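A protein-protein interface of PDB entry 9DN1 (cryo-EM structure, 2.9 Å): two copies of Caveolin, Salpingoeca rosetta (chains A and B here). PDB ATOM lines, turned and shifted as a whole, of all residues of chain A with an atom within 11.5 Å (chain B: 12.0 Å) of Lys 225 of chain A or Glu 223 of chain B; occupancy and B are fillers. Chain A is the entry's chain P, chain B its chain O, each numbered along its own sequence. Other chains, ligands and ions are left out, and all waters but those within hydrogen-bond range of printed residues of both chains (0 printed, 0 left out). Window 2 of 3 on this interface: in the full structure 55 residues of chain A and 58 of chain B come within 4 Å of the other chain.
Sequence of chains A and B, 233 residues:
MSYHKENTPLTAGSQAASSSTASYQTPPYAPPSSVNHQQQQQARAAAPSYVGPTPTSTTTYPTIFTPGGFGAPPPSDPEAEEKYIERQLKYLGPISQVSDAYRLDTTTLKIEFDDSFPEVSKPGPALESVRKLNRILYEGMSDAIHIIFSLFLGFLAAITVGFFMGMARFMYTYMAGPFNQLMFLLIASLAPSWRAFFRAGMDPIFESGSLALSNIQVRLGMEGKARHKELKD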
ATOM      1  N   MET A 222     -22.101 -26.889 -24.285  1.00  0.00           N
ATOM      2  CA  MET A 222     -20.876 -26.121 -24.480  1.00  0.00           C
ATOM      3  C   MET A 222     -21.116 -24.617 -24.413  1.00  0.00           C
ATOM      4  O   MET A 222     -22.179 -24.126 -24.800  1.00  0.00           O
ATOM      5  CB  MET A 222     -20.242 -26.466 -25.832  1.00  0.00           C
ATOM      6  CG  MET A 222     -19.766 -27.905 -25.937  1.00  0.00           C
ATOM      7  SD  MET A 222     -19.259 -28.364 -27.605  1.00  0.00           S
ATOM      8  CE  MET A 222     -20.823 -28.892 -28.300  1.00  0.00           C
ATOM      9  N   GLU A 223     -20.107 -23.899 -23.917  1.00  0.00           N
ATOM     10  CA  GLU A 223     -19.998 -22.446 -23.994  1.00  0.00           C
ATOM     11  C   GLU A 223     -18.621 -22.092 -24.538  1.00  0.00           C
ATOM     12  O   GLU A 223     -17.649 -22.809 -24.282  1.00  0.00           O
ATOM     13  CB  GLU A 223     -20.182 -21.787 -22.621  1.00  0.00           C
ATOM     14  CG  GLU A 223     -21.602 -21.769 -22.092  1.00  0.00           C
ATOM     15  CD  GLU A 223     -22.479 -20.758 -22.798  1.00  0.00           C
ATOM     16  OE1 GLU A 223     -21.933 -19.822 -23.417  1.00  0.00           O
ATOM     17  OE2 GLU A 223     -23.717 -20.893 -22.726  1.00  0.00           O
ATOM     18  N   GLY A 224     -18.526 -20.991 -25.283  1.00  0.00           N
ATOM     19  CA  GLY A 224     -17.235 -20.604 -25.823  1.00  0.00           C
ATOM     20  C   GLY A 224     -17.064 -19.153 -26.223  1.00  0.00           C
ATOM     21  O   GLY A 224     -18.002 -18.510 -26.702  1.00  0.00           O
ATOM     22  N   LYS A 225     -15.852 -18.634 -26.024  1.00  0.00           N
ATOM     23  CA  LYS A 225     -15.429 -17.327 -26.510  1.00  0.00           C
ATOM     24  C   LYS A 225     -14.126 -17.488 -27.279  1.00  0.00           C
ATOM     25  O   LYS A 225     -13.294 -18.328 -26.925  1.00  0.00           O
ATOM     26  CB  LYS A 225     -15.214 -16.336 -25.365  1.00  0.00           C
ATOM     27  CG  LYS A 225     -16.470 -15.689 -24.825  1.00  0.00           C
ATOM     28  CD  LYS A 225     -16.253 -15.127 -23.422  1.00  0.00           C
ATOM     29  CE  LYS A 225     -15.057 -14.182 -23.343  1.00  0.00           C
ATOM     30  NZ  LYS A 225     -15.302 -12.905 -24.060  1.00  0.00           N
ATOM     31  N   ALA A 226     -13.940 -16.680 -28.322  1.00  0.00           N
ATOM     32  CA  ALA A 226     -12.741 -16.774 -29.142  1.00  0.00           C
ATOM     33  C   ALA A 226     -12.323 -15.400 -29.644  1.00  0.00           C
ATOM     34  O   ALA A 226     -13.167 -14.544 -29.914  1.00  0.00           O
ATOM     35  CB  ALA A 226     -12.958 -17.715 -30.330  1.00  0.00           C
ATOM     36  N   ARG A 227     -11.011 -15.203 -29.759  1.00  0.00           N
ATOM     37  CA  ARG A 227     -10.416 -14.012 -30.347  1.00  0.00           C
ATOM     38  C   ARG A 227      -9.324 -14.453 -31.307  1.00  0.00           C
ATOM     39  O   ARG A 227      -8.638 -15.446 -31.051  1.00  0.00           O
ATOM     40  CB  ARG A 227      -9.831 -13.091 -29.268  1.00  0.00           C
ATOM     41  CG  ARG A 227     -10.870 -12.380 -28.420  1.00  0.00           C
ATOM     42  CD  ARG A 227     -10.666 -12.650 -26.937  1.00  0.00           C
ATOM     43  NE  ARG A 227      -9.551 -11.897 -26.375  1.00  0.00           N
ATOM     44  CZ  ARG A 227      -8.776 -12.322 -25.384  1.00  0.00           C
ATOM     45  NH1 ARG A 227      -8.951 -13.507 -24.824  1.00  0.00           N
ATOM     46  NH2 ARG A 227      -7.799 -11.534 -24.944  1.00  0.00           N
ATOM     47  N   HIS A 228      -9.154 -13.727 -32.411  1.00  0.00           N
ATOM     48  CA  HIS A 228      -8.165 -14.125 -33.402  1.00  0.00           C
ATOM     49  C   HIS A 228      -7.624 -12.907 -34.140  1.00  0.00           C
ATOM     50  O   HIS A 228      -8.232 -11.835 -34.147  1.00  0.00           O
ATOM     51  CB  HIS A 228      -8.745 -15.139 -34.395  1.00  0.00           C
ATOM     52  CG  HIS A 228      -9.977 -14.667 -35.101  1.00  0.00           C
ATOM     53  ND1 HIS A 228      -9.936 -14.034 -36.324  1.00  0.00           N
ATOM     54  CD2 HIS A 228     -11.285 -14.748 -34.764  1.00  0.00           C
ATOM     55  CE1 HIS A 228     -11.166 -13.740 -36.707  1.00  0.00           C
ATOM     56  NE2 HIS A 228     -12.003 -14.162 -35.777  1.00  0.00           N
ATOM     57  N   ARG B 219     -20.611 -31.033 -19.074  1.00  0.00           N
ATOM     58  CA  ARG B 219     -20.724 -29.583 -19.179  1.00  0.00           C
ATOM     59  C   ARG B 219     -19.334 -29.005 -19.410  1.00  0.00           C
ATOM     60  O   ARG B 219     -18.399 -29.328 -18.672  1.00  0.00           O
ATOM     61  CB  ARG B 219     -21.337 -28.984 -17.913  1.00  0.00           C
ATOM     62  CG  ARG B 219     -22.819 -29.244 -17.745  1.00  0.00           C
ATOM     63  CD  ARG B 219     -23.322 -28.667 -16.435  1.00  0.00           C
ATOM     64  NE  ARG B 219     -24.778 -28.680 -16.356  1.00  0.00           N
ATOM     65  CZ  ARG B 219     -25.562 -27.651 -16.652  1.00  0.00           C
ATOM     66  NH1 ARG B 219     -25.065 -26.486 -17.037  1.00  0.00           N
ATOM     67  NH2 ARG B 219     -26.881 -27.795 -16.561  1.00  0.00           N
ATOM     68  N   LEU B 220     -19.198 -28.148 -20.423  1.00  0.00           N
ATOM     69  CA  LEU B 220     -17.894 -27.689 -20.879  1.00  0.00           C
ATOM     70  C   LEU B 220     -17.911 -26.191 -21.156  1.00  0.00           C
ATOM     71  O   LEU B 220     -18.897 -25.657 -21.672  1.00  0.00           O
ATOM     72  CB  LEU B 220     -17.476 -28.461 -22.138  1.00  0.00           C
ATOM     73  CG  LEU B 220     -16.242 -28.015 -22.923  1.00  0.00           C
ATOM     74  CD1 LEU B 220     -14.992 -28.059 -22.069  1.00  0.00           C
ATOM     75  CD2 LEU B 220     -16.078 -28.898 -24.145  1.00  0.00           C
ATOM     76  N   GLY B 221     -16.821 -25.523 -20.807  1.00  0.00           N
ATOM     77  CA  GLY B 221     -16.656 -24.108 -21.105  1.00  0.00           C
ATOM     78  C   GLY B 221     -15.242 -23.820 -21.566  1.00  0.00           C
ATOM     79  O   GLY B 221     -14.291 -24.441 -21.098  1.00  0.00           O
ATOM     80  N   MET B 222     -15.112 -22.857 -22.484  1.00  0.00           N
ATOM     81  CA  MET B 222     -13.869 -22.660 -23.221  1.00  0.00           C
ATOM     82  C   MET B 222     -13.501 -21.187 -23.356  1.00  0.00           C
ATOM     83  O   MET B 222     -14.374 -20.319 -23.444  1.00  0.00           O
ATOM     84  CB  MET B 222     -13.980 -23.279 -24.618  1.00  0.00           C
ATOM     85  CG  MET B 222     -14.775 -24.572 -24.653  1.00  0.00           C
ATOM     86  SD  MET B 222     -14.485 -25.553 -26.135  1.00  0.00           S
ATOM     87  CE  MET B 222     -16.144 -25.635 -26.805  1.00  0.00           C
ATOM     88  N   GLU B 223     -12.193 -20.925 -23.372  1.00  0.00           N
ATOM     89  CA  GLU B 223     -11.603 -19.645 -23.749  1.00  0.00           C
ATOM     90  C   GLU B 223     -10.514 -19.902 -24.783  1.00  0.00           C
ATOM     91  O   GLU B 223      -9.844 -20.936 -24.734  1.00  0.00           O
ATOM     92  CB  GLU B 223     -10.992 -18.921 -22.543  1.00  0.00           C
ATOM     93  CG  GLU B 223     -11.987 -18.308 -21.578  1.00  0.00           C
ATOM     94  CD  GLU B 223     -12.640 -17.058 -22.125  1.00  0.00           C
ATOM     95  OE1 GLU B 223     -12.084 -16.456 -23.066  1.00  0.00           O
ATOM     96  OE2 GLU B 223     -13.706 -16.669 -21.608  1.00  0.00           O
ATOM     97  N   GLY B 224     -10.328 -18.967 -25.715  1.00  0.00           N
ATOM     98  CA  GLY B 224      -9.298 -19.158 -26.719  1.00  0.00           C
ATOM     99  C   GLY B 224      -8.780 -17.916 -27.417  1.00  0.00           C
ATOM    100  O   GLY B 224      -9.527 -16.967 -27.667  1.00  0.00           O
ATOM    101  N   LYS B 225      -7.486 -17.926 -27.738  1.00  0.00           N
ATOM    102  CA  LYS B 225      -6.842 -16.923 -28.576  1.00  0.00           C
ATOM    103  C   LYS B 225      -6.096 -17.630 -29.698  1.00  0.00           C
ATOM    104  O   LYS B 225      -5.576 -18.732 -29.503  1.00  0.00           O
ATOM    105  CB  LYS B 225      -5.854 -16.068 -27.780  1.00  0.00           C
ATOM    106  CG  LYS B 225      -6.472 -14.947 -26.973  1.00  0.00           C
ATOM    107  CD  LYS B 225      -5.541 -14.475 -25.858  1.00  0.00           C
ATOM    108  CE  LYS B 225      -4.152 -14.097 -26.367  1.00  0.00           C
ATOM    109  NZ  LYS B 225      -4.172 -12.856 -27.181  1.00  0.00           N
ATOM    110  N   ALA B 226      -6.033 -16.998 -30.869  1.00  0.00           N
ATOM    111  CA  ALA B 226      -5.371 -17.602 -32.017  1.00  0.00           C
ATOM    112  C   ALA B 226      -4.713 -16.538 -32.881  1.00  0.00           C
ATOM    113  O   ALA B 226      -5.228 -15.425 -33.013  1.00  0.00           O
ATOM    114  CB  ALA B 226      -6.361 -18.413 -32.858  1.00  0.00           C
ATOM    115  N   ARG B 227      -3.569 -16.893 -33.463  1.00  0.00           N
ATOM    116  CA  ARG B 227      -2.857 -16.069 -34.428  1.00  0.00           C
ATOM    117  C   ARG B 227      -2.463 -16.951 -35.603  1.00  0.00           C
ATOM    118  O   ARG B 227      -2.146 -18.127 -35.415  1.00  0.00           O
ATOM    119  CB  ARG B 227      -1.610 -15.430 -33.804  1.00  0.00           C
ATOM    120  CG  ARG B 227      -1.906 -14.329 -32.800  1.00  0.00           C
ATOM    121  CD  ARG B 227      -1.260 -14.608 -31.450  1.00  0.00           C
ATOM    122  NE  ARG B 227       0.176 -14.355 -31.447  1.00  0.00           N
ATOM    123  CZ  ARG B 227       1.061 -15.023 -30.718  1.00  0.00           C
ATOM    124  NH1 ARG B 227       0.696 -16.015 -29.920  1.00  0.00           N
ATOM    125  NH2 ARG B 227       2.344 -14.686 -30.787  1.00  0.00           N
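Hydrophobic or aromatic side chains of chain A that line the printed part of chain B: His 228. Printed residues of chain B that touch a printed residue of chain A: Leu 220, Gly 221, Met 222, Glu 223, Gly 224, Lys 225 and Ala 226. Among the printed residues, 13 pairs touch across the chains.
Among the printed residues, merely in contact across the chains: Met 222 of chain A with Leu 220 of chain B, Glu 223 of chain A with Gly 221 of chain B, Gly 224 of chain A with Met 222 of chain B, Lys 225 of chain A with Glu 223 of chain B, Ala 226 of chain A with Gly 224 of chain B, Arg 227 of chain A with Lys 225 of chain B and His 228 of chain A with Ala 226 of chain B.
Gly 224 of chain A touches Met 222 of chain B, but with the chains exchanged Met 222 of chain A does not touch Gly 224 of chain B (12.2 Å). Lys 225 of chain A touches Met 222 of chain B, but with the chains exchanged Met 222 of chain A does not touch Lys 225 of chain B (15.5 Å). Ala 226 of chain A touches Gly 224 of chain B, but with the chains exchanged Gly 224 of chain A does not touch Ala 226 of chain B (12.2 Å). Arg 227 of chain A touches Lys 225 of chain B, but with the chains exchanged Lys 225 of chain A does not touch Arg 227 of chain B (11.8 Å). Positions printed for both chains: 222, 223, 224, 225, 226 and 227.
O of Leu 220 of chain B sits at hydrogen-bond distance from N of Glu 223 of chain A, 3.1 Å away. N of Met 222 of chain B lies within hydrogen-bond range of O of Glu 223 of chain A (3.1 Å). The backbone NH (N) of Lys 225 of chain A is in hydrogen-bond range of the backbone carbonyl oxygen (O) of Met 222 of chain B, 3.4 Å away. N of Gly 224 of chain B is in hydrogen-bond range of O of Lys 225 of chain A, at 3.3 Å. The backbone carbonyl oxygen of Gly 224 of chain B is in hydrogen-bond range of the backbone NH of Arg 227 of chain A. N of Ala 226 of chain B sits at hydrogen-bond distance from O of Arg 227 of chain A (3.0 Å).
Printed residues of chain B within 4 Å of Glu 223 of chain A: Leu 220, Gly 221 and Met 222. Printed residues of chain B within 4 Å of Lys 225 of chain A: Met 222 (3.4 Å), Glu 223 (3.3 Å) and Gly 224 (3.3 Å). Of chain B, only Gly 224 comes within 4 Å of Ala 226 of chain A. Of the printed residues of chain B, Arg 227 of chain A touches Gly 224 (3.1 Å), Lys 225 (3.4 Å) and Ala 226 (3.0 Å). Of chain A, only Glu 223 (3.6 Å) comes within 4 Å of Gly 221 of chain B. Met 222 of chain B touches just these residues of chain A: Glu 223, Gly 224 and Lys 225. Of chain A, only Lys 225 (3.3 Å) comes within 4 Å of Glu 223 of chain B. Gly 224 of chain B touches just these residues of chain A: Lys 225, Ala 226 and Arg 227. Of the printed residues of chain A, Ala 226 of chain B touches Arg 227 and His 228. The nearest residue of chain A that does not touch Glu 223 of chain B is Arg 227 of chain A (4.6 Å).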
